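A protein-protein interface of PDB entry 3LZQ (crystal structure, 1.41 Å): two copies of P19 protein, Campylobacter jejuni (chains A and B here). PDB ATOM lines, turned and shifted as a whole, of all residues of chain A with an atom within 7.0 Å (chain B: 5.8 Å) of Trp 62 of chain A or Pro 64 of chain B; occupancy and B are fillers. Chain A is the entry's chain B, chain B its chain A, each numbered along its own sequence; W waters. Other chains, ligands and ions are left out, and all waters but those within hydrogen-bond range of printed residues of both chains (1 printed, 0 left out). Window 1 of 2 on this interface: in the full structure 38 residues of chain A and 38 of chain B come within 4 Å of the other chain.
The side-chain hydroxyl of Tyr 65 of chain B is in hydrogen-bond range of the backbone NH of Tyr 65 of chain A (2.9 Å).
The backbone NH (N) of Ala 49 of chain A lies within hydrogen-bond range of the backbone carbonyl oxygen (O) of Phe 61 of chain A (2.9 Å). The backbone NH (N) of Tyr 65 of chain A sits at hydrogen-bond distance from the side-chain hydroxyl (OH) of Tyr 96 of chain A, 3.2 Å away. N of Tyr 65 of chain B is in hydrogen-bond range of OH of Tyr 96 of chain B (3.2 Å). O of Pro 124 of chain B sits close to N of Phe 129 of chain B, at 3.3 Å. The backbone carbonyl oxygen (O) of Ala 49 of chain A lies within hydrogen-bond range of the backbone NH (N) of Gly 60 of chain A, 2.9 Å away.
CZ of Phe 61 of chain B touches O of Gly 60 of chain A (3.3 Å). Trp 62 of chain B touches Phe 61 of chain A (N to CZ, 3.9 Å). Trp 62 of chain A touches Phe 61 of chain B (N to CE2, 3.8 Å). Trp 62 of chain A touches Pro 64 of chain B. Trp 62 of chain A touches Phe 129 of chain B (CH2 to CE2, 3.95 Å). Pro 64 of chain A touches Trp 62 of chain B. Pro 87 of chain A touches Tyr 65 of chain B (CB to OH, 3.6 Å). CA of Phe 129 of chain B touches O of Pro 87 of chain A, at 3.6 Å. Met 88 of chain A touches Phe 129 of chain B. Phe 57 of chain B touches Pro 94 of chain A.
Of chain B, only Phe 61, Pro 64, Tyr 65 and Phe 129 come within 4 Å of Trp 62 of chain A. Pro 64 of chain B touches one residue of chain A. Of the printed residues of chain A, Tyr 65 of chain B touches Trp 62 (3.7 Å), Tyr 65 (2.9 Å) and Pro 87 (3.6 Å). Of the printed residues of chain A, Trp 62 of chain B touches Phe 61 (3.9 Å), Pro 64 (3.8 Å) and Tyr 65 (3.8 Å). Tyr 96 of chain A touches none of the printed residues of chain B. The nearest residue of chain B that does not touch Trp 62 of chain A is Phe 57 of chain B (5.1 Å). The nearest printed residue of chain B that does not touch Tyr 65 of chain A is Tyr 96 of chain B (4.1 Å).
Of the 10 printed residues of chain B, 6 touch a printed residue of chain A. Hydrophobic or aromatic side chains of chain B that line the printed part of chain A: Phe 57, Phe 61, Trp 62, Pro 64, Tyr 65 and Phe 129. Along chain B the printed residues that touch a printed residue of chain A span positions 57 to 129. Hydrophobic or aromatic side chains of chain A within 4 Å of the printed part of chain B: Phe 61, Trp 62, Pro 64, Tyr 65, Pro 87 and Pro 94. Among the printed residues, 13 pairs touch across the chains. Among the printed residues, no Asp or Glu carboxylate lies within 4 Å of a Lys or Arg side-chain nitrogen of the other chain.
Phe 61 of chain A touches Trp 62 of chain B, and with the chains exchanged Trp 62 of chain A touches Phe 61 of chain B. Trp 62 of chain A touches Pro 64 of chain B, and with the chains exchanged Pro 64 of chain A touches Trp 62 of chain B. Trp 62 of chain A touches Tyr 65 of chain B, and with the chains exchanged Tyr 65 of chain A touches Trp 62 of chain B. Tyr 65 of chain A touches its own counterpart, Tyr 65 of chain B. Positions printed for both chains: 57, 61, 62, 63, 64, 65, 66 and 96. Of the 13 pairs that touch across the chains among the printed residues, 7 have their exchanged pair printed and touching as well.
Water W1 lies within hydrogen-bond range of the side-chain hydroxyl of Tyr 65 of chain A (2.5 Å) and the backbone carbonyl oxygen of Leu 66 of chain B (3.1 Å).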
ATOM      1  N   ALA A  45     -17.196   3.062  -1.286  1.00  0.00           N
ATOM      2  CA  ALA A  45     -17.425   2.391  -0.030  1.00  0.00           C
ATOM      3  C   ALA A  45     -16.452   2.996   0.965  1.00  0.00           C
ATOM      4  O   ALA A  45     -15.219   3.009   0.710  1.00  0.00           O
ATOM      5  CB  ALA A  45     -17.152   0.874  -0.141  1.00  0.00           C
ATOM      6  N   ASP A  46     -17.007   3.482   2.079  1.00  0.00           N
ATOM      7  CA  ASP A  46     -16.258   4.079   3.183  1.00  0.00           C
ATOM      8  C   ASP A  46     -16.269   3.085   4.331  1.00  0.00           C
ATOM      9  O   ASP A  46     -17.321   2.807   4.922  1.00  0.00           O
ATOM     10  CB  ASP A  46     -16.918   5.399   3.557  1.00  0.00           C
ATOM     11  CG  ASP A  46     -16.627   6.508   2.545  1.00  0.00           C
ATOM     12  OD1 ASP A  46     -15.565   6.489   1.868  1.00  0.00           O
ATOM     13  OD2 ASP A  46     -17.463   7.417   2.446  1.00  0.00           O
ATOM     14  N   ILE A  47     -15.100   2.509   4.628  1.00  0.00           N
ATOM     15  CA  ILE A  47     -14.976   1.441   5.603  1.00  0.00           C
ATOM     16  C   ILE A  47     -13.839   1.711   6.586  1.00  0.00           C
ATOM     17  O   ILE A  47     -12.675   1.762   6.195  1.00  0.00           O
ATOM     18  CB  ILE A  47     -14.691   0.114   4.905  1.00  0.00           C
ATOM     19  CG1 ILE A  47     -15.733  -0.097   3.817  1.00  0.00           C
ATOM     20  CG2 ILE A  47     -14.722  -1.048   5.886  1.00  0.00           C
ATOM     21  CD1 ILE A  47     -15.652  -1.422   3.113  1.00  0.00           C
ATOM     22  N   HIS A  48     -14.195   1.884   7.854  1.00  0.00           N
ATOM     23  CA  HIS A  48     -13.246   2.247   8.908  1.00  0.00           C
ATOM     24  C   HIS A  48     -13.484   1.401  10.141  1.00  0.00           C
ATOM     25  O   HIS A  48     -14.597   0.925  10.377  1.00  0.00           O
ATOM     26  CB  HIS A  48     -13.370   3.754   9.260  1.00  0.00           C
ATOM     27  CG  HIS A  48     -13.051   4.653   8.107  1.00  0.00           C
ATOM     28  ND1 HIS A  48     -13.988   4.940   7.135  1.00  0.00           N
ATOM     29  CD2 HIS A  48     -11.908   5.278   7.733  1.00  0.00           C
ATOM     30  CE1 HIS A  48     -13.424   5.705   6.210  1.00  0.00           C
ATOM     31  NE2 HIS A  48     -12.161   5.920   6.547  1.00  0.00           N
ATOM     32  N   ALA A  49     -12.443   1.247  10.972  1.00  0.00           N
ATOM     33  CA  ALA A  49     -12.562   0.501  12.212  1.00  0.00           C
ATOM     34  C   ALA A  49     -13.389   1.207  13.256  1.00  0.00           C
ATOM     35  O   ALA A  49     -13.342   2.432  13.408  1.00  0.00           O
ATOM     36  CB  ALA A  49     -11.212   0.167  12.777  1.00  0.00           C
ATOM     37  N   PHE A  57      -7.141  -2.966  14.584  1.00  0.00           N
ATOM     38  CA  PHE A  57      -7.157  -1.663  13.941  1.00  0.00           C
ATOM     39  C   PHE A  57      -7.661  -0.593  14.874  1.00  0.00           C
ATOM     40  O   PHE A  57      -8.746  -0.784  15.472  1.00  0.00           O
ATOM     41  CB  PHE A  57      -7.973  -1.736  12.647  1.00  0.00           C
ATOM     42  CG  PHE A  57      -7.176  -2.276  11.490  1.00  0.00           C
ATOM     43  CD1 PHE A  57      -6.997  -3.633  11.303  1.00  0.00           C
ATOM     44  CD2 PHE A  57      -6.529  -1.401  10.625  1.00  0.00           C
ATOM     45  CE1 PHE A  57      -6.232  -4.099  10.250  1.00  0.00           C
ATOM     46  CE2 PHE A  57      -5.776  -1.878   9.575  1.00  0.00           C
ATOM     47  CZ  PHE A  57      -5.614  -3.230   9.413  1.00  0.00           C
ATOM     48  N   PRO A  58      -6.874   0.501  15.054  1.00  0.00           N
ATOM     49  CA  PRO A  58      -7.347   1.636  15.860  1.00  0.00           C
ATOM     50  C   PRO A  58      -8.656   2.208  15.335  1.00  0.00           C
ATOM     51  O   PRO A  58      -8.912   2.192  14.131  1.00  0.00           O
ATOM     52  CB  PRO A  58      -6.248   2.688  15.702  1.00  0.00           C
ATOM     53  CG  PRO A  58      -5.018   1.940  15.375  1.00  0.00           C
ATOM     54  CD  PRO A  58      -5.500   0.715  14.558  1.00  0.00           C
ATOM     55  N   GLU A  59      -9.497   2.671  16.255  1.00  0.00           N
ATOM     56  CA  GLU A  59     -10.741   3.306  15.896  1.00  0.00           C
ATOM     57  C   GLU A  59     -10.499   4.375  14.852  1.00  0.00           C
ATOM     58  O   GLU A  59      -9.628   5.213  15.053  1.00  0.00           O
ATOM     59  CB  GLU A  59     -11.401   3.914  17.178  1.00  0.00           C
ATOM     60  CG  GLU A  59     -12.749   4.612  16.872  1.00  0.00           C
ATOM     61  CD  GLU A  59     -13.481   5.167  18.106  1.00  0.00           C
ATOM     62  OE1 GLU A  59     -12.951   5.105  19.217  1.00  0.00           O
ATOM     63  OE2 GLU A  59     -14.586   5.695  17.937  1.00  0.00           O
ATOM     64  N   GLY A  60     -11.301   4.391  13.775  1.00  0.00           N
ATOM     65  CA  GLY A  60     -11.183   5.436  12.770  1.00  0.00           C
ATOM     66  C   GLY A  60     -10.270   5.099  11.610  1.00  0.00           C
ATOM     67  O   GLY A  60     -10.312   5.776  10.561  1.00  0.00           O
ATOM     68  N   PHE A  61      -9.364   4.137  11.804  1.00  0.00           N
ATOM     69  CA  PHE A  61      -8.457   3.764  10.710  1.00  0.00           C
ATOM     70  C   PHE A  61      -9.227   3.233   9.509  1.00  0.00           C
ATOM     71  O   PHE A  61     -10.168   2.464   9.666  1.00  0.00           O
ATOM     72  CB  PHE A  61      -7.406   2.733  11.107  1.00  0.00           C
ATOM     73  CG  PHE A  61      -6.089   3.295  11.568  1.00  0.00           C
ATOM     74  CD1 PHE A  61      -5.942   4.582  12.067  1.00  0.00           C
ATOM     75  CD2 PHE A  61      -4.950   2.513  11.416  1.00  0.00           C
ATOM     76  CE1 PHE A  61      -4.694   5.059  12.479  1.00  0.00           C
ATOM     77  CE2 PHE A  61      -3.721   2.978  11.805  1.00  0.00           C
ATOM     78  CZ  PHE A  61      -3.581   4.246  12.320  1.00  0.00           C
ATOM     79  N   TRP A  62      -8.759   3.556   8.322  1.00  0.00           N
ATOM     80  CA  TRP A  62      -9.279   2.921   7.127  1.00  0.00           C
ATOM     81  C   TRP A  62      -8.941   1.427   7.157  1.00  0.00           C
ATOM     82  O   TRP A  62      -7.830   1.050   7.548  1.00  0.00           O
ATOM     83  CB  TRP A  62      -8.610   3.566   5.900  1.00  0.00           C
ATOM     84  CG  TRP A  62      -9.105   3.046   4.598  1.00  0.00           C
ATOM     85  CD1 TRP A  62     -10.374   3.067   4.166  1.00  0.00           C
ATOM     86  CD2 TRP A  62      -8.320   2.502   3.531  1.00  0.00           C
ATOM     87  NE1 TRP A  62     -10.470   2.533   2.904  1.00  0.00           N
ATOM     88  CE2 TRP A  62      -9.219   2.161   2.494  1.00  0.00           C
ATOM     89  CE3 TRP A  62      -6.947   2.253   3.353  1.00  0.00           C
ATOM     90  CZ2 TRP A  62      -8.800   1.620   1.287  1.00  0.00           C
ATOM     91  CZ3 TRP A  62      -6.527   1.708   2.150  1.00  0.00           C
ATOM     92  CH2 TRP A  62      -7.463   1.350   1.150  1.00  0.00           C
ATOM     93  N   MET A  63      -9.854   0.587   6.655  1.00  0.00           N
ATOM     94  CA  MET A  63      -9.617  -0.851   6.586  1.00  0.00           C
ATOM     95  C   MET A  63      -9.062  -1.183   5.216  1.00  0.00           C
ATOM     96  O   MET A  63      -9.822  -1.113   4.253  1.00  0.00           O
ATOM     97  CB  MET A  63     -10.913  -1.614   6.796  1.00  0.00           C
ATOM     98  CG  MET A  63     -11.589  -1.374   8.113  1.00  0.00           C
ATOM     99  SD  MET A  63     -10.608  -1.814   9.565  1.00  0.00           S
ATOM    100  CE  MET A  63     -10.355  -3.597   9.336  1.00  0.00           C
ATOM    101  N   PRO A  64      -7.762  -1.550   5.130  1.00  0.00           N
ATOM    102  CA  PRO A  64      -7.069  -1.699   3.851  1.00  0.00           C
ATOM    103  C   PRO A  64      -7.096  -3.141   3.360  1.00  0.00           C
ATOM    104  O   PRO A  64      -7.332  -4.070   4.155  1.00  0.00           O
ATOM    105  CB  PRO A  64      -5.636  -1.277   4.211  1.00  0.00           C
ATOM    106  CG  PRO A  64      -5.444  -1.899   5.570  1.00  0.00           C
ATOM    107  CD  PRO A  64      -6.807  -1.733   6.257  1.00  0.00           C
ATOM    108  N   TYR A  65      -6.775  -3.347   2.094  1.00  0.00           N
ATOM    109  CA  TYR A  65      -6.672  -4.671   1.482  1.00  0.00           C
ATOM    110  C   TYR A  65      -7.967  -5.508   1.497  1.00  0.00           C
ATOM    111  O   TYR A  65      -7.934  -6.743   1.348  1.00  0.00           O
ATOM    112  CB  TYR A  65      -5.521  -5.477   2.079  1.00  0.00           C
ATOM    113  CG  TYR A  65      -4.155  -4.805   2.005  1.00  0.00           C
ATOM    114  CD1 TYR A  65      -3.294  -5.025   0.937  1.00  0.00           C
ATOM    115  CD2 TYR A  65      -3.709  -4.011   3.026  1.00  0.00           C
ATOM    116  CE1 TYR A  65      -2.047  -4.408   0.871  1.00  0.00           C
ATOM    117  CE2 TYR A  65      -2.503  -3.419   2.987  1.00  0.00           C
ATOM    118  CZ  TYR A  65      -1.657  -3.591   1.909  1.00  0.00           C
ATOM    119  OH  TYR A  65      -0.436  -2.994   1.978  1.00  0.00           O
ATOM    120  N   LEU A  66      -9.112  -4.852   1.647  1.00  0.00           N
ATOM    121  CA  LEU A  66     -10.367  -5.559   1.536  1.00  0.00           C
ATOM    122  C   LEU A  66     -10.660  -5.829   0.053  1.00  0.00           C
ATOM    123  O   LEU A  66     -10.277  -5.060  -0.832  1.00  0.00           O
ATOM    124  CB  LEU A  66     -11.531  -4.744   2.102  1.00  0.00           C
ATOM    125  CG  LEU A  66     -11.443  -4.432   3.584  1.00  0.00           C
ATOM    126  CD1 LEU A  66     -12.569  -3.465   3.978  1.00  0.00           C
ATOM    127  CD2 LEU A  66     -11.561  -5.738   4.429  1.00  0.00           C
ATOM    128  N   MET A  86     -12.093  -0.454  -6.233  1.00  0.00           N
ATOM    129  CA  MET A  86     -10.638  -0.487  -6.121  1.00  0.00           C
ATOM    130  C   MET A  86     -10.182   0.516  -5.086  1.00  0.00           C
ATOM    131  O   MET A  86     -10.801   1.541  -4.913  1.00  0.00           O
ATOM    132  CB  MET A  86      -9.939  -0.189  -7.464  1.00  0.00           C
ATOM    133  CG  MET A  86     -10.138   1.204  -8.037  1.00  0.00           C
ATOM    134  SD  MET A  86      -9.051   1.614  -9.416  1.00  0.00           S
ATOM    135  CE  MET A  86      -7.715   2.370  -8.486  1.00  0.00           C
ATOM    136  N   PRO A  87      -9.093   0.218  -4.409  1.00  0.00           N
ATOM    137  CA  PRO A  87      -8.576   1.153  -3.403  1.00  0.00           C
ATOM    138  C   PRO A  87      -7.933   2.358  -4.039  1.00  0.00           C
ATOM    139  O   PRO A  87      -7.275   2.244  -5.059  1.00  0.00           O
ATOM    140  CB  PRO A  87      -7.524   0.315  -2.662  1.00  0.00           C
ATOM    141  CG  PRO A  87      -7.018  -0.586  -3.699  1.00  0.00           C
ATOM    142  CD  PRO A  87      -8.220  -0.958  -4.538  1.00  0.00           C
ATOM    143  N   MET A  88      -8.157   3.517  -3.433  1.00  0.00           N
ATOM    144  CA  MET A  88      -7.643   4.740  -3.952  1.00  0.00           C
ATOM    145  C   MET A  88      -7.702   5.809  -2.878  1.00  0.00           C
ATOM    146  O   MET A  88      -8.287   5.633  -1.819  1.00  0.00           O
ATOM    147  CB  MET A  88      -8.474   5.168  -5.174  1.00  0.00           C
ATOM    148  CG  MET A  88      -9.887   5.567  -4.866  1.00  0.00           C
ATOM    149  SD  MET A  88     -10.867   5.930  -6.353  1.00  0.00           S
ATOM    150  CE  MET A  88     -11.039   4.238  -7.031  1.00  0.00           C
ATOM    151  N   GLY A  93      -8.876  11.424   2.062  1.00  0.00           N
ATOM    152  CA  GLY A  93      -8.369  10.121   2.492  1.00  0.00           C
ATOM    153  C   GLY A  93      -8.704   8.946   1.622  1.00  0.00           C
ATOM    154  O   GLY A  93      -9.405   9.067   0.599  1.00  0.00           O
ATOM    155  N   PRO A  94      -8.202   7.753   2.033  1.00  0.00           N
ATOM    156  CA  PRO A  94      -8.429   6.555   1.225  1.00  0.00           C
ATOM    157  C   PRO A  94      -9.881   6.018   1.283  1.00  0.00           C
ATOM    158  O   PRO A  94     -10.594   6.216   2.277  1.00  0.00           O
ATOM    159  CB  PRO A  94      -7.438   5.546   1.841  1.00  0.00           C
ATOM    160  CG  PRO A  94      -7.335   6.000   3.325  1.00  0.00           C
ATOM    161  CD  PRO A  94      -7.377   7.495   3.230  1.00  0.00           C
ATOM    162  N   HIS A  95     -10.302   5.355   0.196  1.00  0.00           N
ATOM    163  CA  HIS A  95     -11.575   4.665   0.128  1.00  0.00           C
ATOM    164  C   HIS A  95     -11.485   3.604  -0.974  1.00  0.00           C
ATOM    165  O   HIS A  95     -10.426   3.396  -1.592  1.00  0.00           O
ATOM    166  CB  HIS A  95     -12.719   5.660  -0.173  1.00  0.00           C
ATOM    167  CG  HIS A  95     -12.542   6.397  -1.459  1.00  0.00           C
ATOM    168  ND1 HIS A  95     -11.937   7.633  -1.533  1.00  0.00           N
ATOM    169  CD2 HIS A  95     -12.890   6.074  -2.718  1.00  0.00           C
ATOM    170  CE1 HIS A  95     -11.906   8.026  -2.789  1.00  0.00           C
ATOM    171  NE2 HIS A  95     -12.468   7.095  -3.528  1.00  0.00           N
ATOM    172  N   TYR A  96     -12.586   2.902  -1.194  1.00  0.00           N
ATOM    173  CA  TYR A  96     -12.711   1.994  -2.329  1.00  0.00           C
ATOM    174  C   TYR A  96     -13.758   2.569  -3.287  1.00  0.00           C
ATOM    175  O   TYR A  96     -14.763   3.095  -2.868  1.00  0.00           O
ATOM    176  CB  TYR A  96     -13.134   0.611  -1.868  1.00  0.00           C
ATOM    177  CG  TYR A  96     -12.212  -0.025  -0.874  1.00  0.00           C
ATOM    178  CD1 TYR A  96     -12.383   0.151   0.492  1.00  0.00           C
ATOM    179  CD2 TYR A  96     -11.196  -0.864  -1.290  1.00  0.00           C
ATOM    180  CE1 TYR A  96     -11.537  -0.481   1.407  1.00  0.00           C
ATOM    181  CE2 TYR A  96     -10.367  -1.471  -0.401  1.00  0.00           C
ATOM    182  CZ  TYR A  96     -10.509  -1.275   0.946  1.00  0.00           C
ATOM    183  OH  TYR A  96      -9.630  -1.914   1.806  1.00  0.00           O
ATOM    184  N   PHE B  57      -3.605  11.535   2.622  1.00  0.00           N
ATOM    185  CA  PHE B  57      -3.789  10.663   3.792  1.00  0.00           C
ATOM    186  C   PHE B  57      -3.899  11.478   5.075  1.00  0.00           C
ATOM    187  O   PHE B  57      -3.062  12.336   5.316  1.00  0.00           O
ATOM    188  CB  PHE B  57      -2.644   9.661   3.912  1.00  0.00           C
ATOM    189  CG  PHE B  57      -2.871   8.469   3.071  1.00  0.00           C
ATOM    190  CD1 PHE B  57      -2.531   8.489   1.726  1.00  0.00           C
ATOM    191  CD2 PHE B  57      -3.481   7.330   3.621  1.00  0.00           C
ATOM    192  CE1 PHE B  57      -2.807   7.358   0.931  1.00  0.00           C
ATOM    193  CE2 PHE B  57      -3.726   6.217   2.839  1.00  0.00           C
ATOM    194  CZ  PHE B  57      -3.406   6.265   1.503  1.00  0.00           C
ATOM    195  N   PHE B  61      -2.647   8.375   9.864  1.00  0.00           N
ATOM    196  CA  PHE B  61      -3.125   7.148   9.234  1.00  0.00           C
ATOM    197  C   PHE B  61      -1.884   6.329   8.848  1.00  0.00           C
ATOM    198  O   PHE B  61      -0.872   6.876   8.397  1.00  0.00           O
ATOM    199  CB  PHE B  61      -3.972   7.425   7.974  1.00  0.00           C
ATOM    200  CG  PHE B  61      -5.442   7.404   8.185  1.00  0.00           C
ATOM    201  CD1 PHE B  61      -5.991   7.719   9.408  1.00  0.00           C
ATOM    202  CD2 PHE B  61      -6.308   7.084   7.110  1.00  0.00           C
ATOM    203  CE1 PHE B  61      -7.357   7.712   9.594  1.00  0.00           C
ATOM    204  CE2 PHE B  61      -7.715   7.069   7.295  1.00  0.00           C
ATOM    205  CZ  PHE B  61      -8.235   7.374   8.545  1.00  0.00           C
ATOM    206  N   TRP B  62      -2.034   5.030   8.871  1.00  0.00           N
ATOM    207  CA  TRP B  62      -1.037   4.095   8.317  1.00  0.00           C
ATOM    208  C   TRP B  62      -0.994   4.281   6.811  1.00  0.00           C
ATOM    209  O   TRP B  62      -2.017   4.506   6.168  1.00  0.00           O
ATOM    210  CB  TRP B  62      -1.466   2.671   8.630  1.00  0.00           C
ATOM    211  CG  TRP B  62      -0.476   1.684   8.175  1.00  0.00           C
ATOM    212  CD1 TRP B  62       0.823   1.582   8.549  1.00  0.00           C
ATOM    213  CD2 TRP B  62      -0.721   0.589   7.279  1.00  0.00           C
ATOM    214  NE1 TRP B  62       1.446   0.550   7.879  1.00  0.00           N
ATOM    215  CE2 TRP B  62       0.500  -0.123   7.147  1.00  0.00           C
ATOM    216  CE3 TRP B  62      -1.860   0.105   6.630  1.00  0.00           C
ATOM    217  CZ2 TRP B  62       0.613  -1.268   6.361  1.00  0.00           C
ATOM    218  CZ3 TRP B  62      -1.734  -1.014   5.816  1.00  0.00           C
ATOM    219  CH2 TRP B  62      -0.519  -1.704   5.704  1.00  0.00           C
ATOM    220  N   MET B  63       0.206   4.258   6.254  1.00  0.00           N
ATOM    221  CA  MET B  63       0.388   4.364   4.821  1.00  0.00           C
ATOM    222  C   MET B  63       0.384   2.988   4.202  1.00  0.00           C
ATOM    223  O   MET B  63       1.370   2.239   4.365  1.00  0.00           O
ATOM    224  CB  MET B  63       1.720   5.033   4.519  1.00  0.00           C
ATOM    225  CG  MET B  63       1.937   6.449   5.002  1.00  0.00           C
ATOM    226  SD  MET B  63       0.672   7.593   4.425  1.00  0.00           S
ATOM    227  CE  MET B  63       1.089   7.649   2.682  1.00  0.00           C
ATOM    228  N   PRO B  64      -0.695   2.634   3.475  1.00  0.00           N
ATOM    229  CA  PRO B  64      -0.912   1.270   2.970  1.00  0.00           C
ATOM    230  C   PRO B  64      -0.410   1.082   1.528  1.00  0.00           C
ATOM    231  O   PRO B  64      -0.134   2.056   0.837  1.00  0.00           O
ATOM    232  CB  PRO B  64      -2.436   1.179   2.992  1.00  0.00           C
ATOM    233  CG  PRO B  64      -2.879   2.523   2.571  1.00  0.00           C
ATOM    234  CD  PRO B  64      -1.832   3.503   3.116  1.00  0.00           C
ATOM    235  N   TYR B  65      -0.321  -0.167   1.100  1.00  0.00           N
ATOM    236  CA  TYR B  65       0.019  -0.572  -0.262  1.00  0.00           C
ATOM    237  C   TYR B  65       1.450  -0.175  -0.712  1.00  0.00           C
ATOM    238  O   TYR B  65       1.748  -0.208  -1.885  1.00  0.00           O
ATOM    239  CB  TYR B  65      -1.027  -0.036  -1.248  1.00  0.00           C
ATOM    240  CG  TYR B  65      -2.400  -0.646  -1.063  1.00  0.00           C
ATOM    241  CD1 TYR B  65      -3.322  -0.079  -0.236  1.00  0.00           C
ATOM    242  CD2 TYR B  65      -2.768  -1.764  -1.754  1.00  0.00           C
ATOM    243  CE1 TYR B  65      -4.544  -0.631  -0.034  1.00  0.00           C
ATOM    244  CE2 TYR B  65      -4.028  -2.334  -1.575  1.00  0.00           C
ATOM    245  CZ  TYR B  65      -4.925  -1.728  -0.727  1.00  0.00           C
ATOM    246  OH  TYR B  65      -6.190  -2.232  -0.531  1.00  0.00           O
ATOM    247  N   LEU B  66       2.343   0.116   0.229  1.00  0.00           N
ATOM    248  CA  LEU B  66       3.739   0.418  -0.118  1.00  0.00           C
ATOM    249  C   LEU B  66       4.469  -0.878  -0.402  1.00  0.00           C
ATOM    250  O   LEU B  66       4.134  -1.919   0.157  1.00  0.00           O
ATOM    251  CB  LEU B  66       4.442   1.110   1.038  1.00  0.00           C
ATOM    252  CG  LEU B  66       3.869   2.453   1.427  1.00  0.00           C
ATOM    253  CD1 LEU B  66       4.634   3.030   2.624  1.00  0.00           C
ATOM    254  CD2 LEU B  66       3.961   3.438   0.258  1.00  0.00           C
ATOM    255  N   TYR B  96       4.526  -2.858   8.537  1.00  0.00           N
ATOM    256  CA  TYR B  96       5.220  -3.691   7.568  1.00  0.00           C
ATOM    257  C   TYR B  96       6.295  -4.367   8.383  1.00  0.00           C
ATOM    258  O   TYR B  96       7.039  -3.678   9.124  1.00  0.00           O
ATOM    259  CB  TYR B  96       5.858  -2.863   6.443  1.00  0.00           C
ATOM    260  CG  TYR B  96       4.864  -2.090   5.606  1.00  0.00           C
ATOM    261  CD1 TYR B  96       4.237  -2.649   4.456  1.00  0.00           C
ATOM    262  CD2 TYR B  96       4.535  -0.808   5.940  1.00  0.00           C
ATOM    263  CE1 TYR B  96       3.304  -1.948   3.714  1.00  0.00           C
ATOM    264  CE2 TYR B  96       3.634  -0.077   5.199  1.00  0.00           C
ATOM    265  CZ  TYR B  96       3.016  -0.640   4.046  1.00  0.00           C
ATOM    266  OH  TYR B  96       2.096  -0.035   3.242  1.00  0.00           O
ATOM    267  N   PRO B 124       2.210   3.388  -3.683  1.00  0.00           N
ATOM    268  CA  PRO B 124       1.142   2.421  -3.826  1.00  0.00           C
ATOM    269  C   PRO B 124       0.691   2.103  -5.233  1.00  0.00           C
ATOM    270  O   PRO B 124       0.005   1.104  -5.413  1.00  0.00           O
ATOM    271  CB  PRO B 124      -0.007   3.095  -3.086  1.00  0.00           C
ATOM    272  CG  PRO B 124       0.674   3.895  -2.040  1.00  0.00           C
ATOM    273  CD  PRO B 124       1.790   4.497  -2.816  1.00  0.00           C
ATOM    274  N   PHE B 129      -3.063   0.786  -6.545  1.00  0.00           N
ATOM    275  CA  PHE B 129      -3.773   1.767  -5.729  1.00  0.00           C
ATOM    276  C   PHE B 129      -3.907   3.026  -6.559  1.00  0.00           C
ATOM    277  O   PHE B 129      -2.932   3.482  -7.152  1.00  0.00           O
ATOM    278  CB  PHE B 129      -2.955   2.053  -4.467  1.00  0.00           C
ATOM    279  CG  PHE B 129      -3.660   2.898  -3.429  1.00  0.00           C
ATOM    280  CD1 PHE B 129      -3.539   4.237  -3.443  1.00  0.00           C
ATOM    281  CD2 PHE B 129      -4.400   2.310  -2.441  1.00  0.00           C
ATOM    282  CE1 PHE B 129      -4.165   4.996  -2.467  1.00  0.00           C
ATOM    283  CE2 PHE B 129      -5.066   3.066  -1.483  1.00  0.00           C
ATOM    284  CZ  PHE B 129      -4.932   4.402  -1.502  1.00  0.00           C
HETATM  285  O   HOH W   1       1.485  -3.572   0.469  1.00  0.00           O
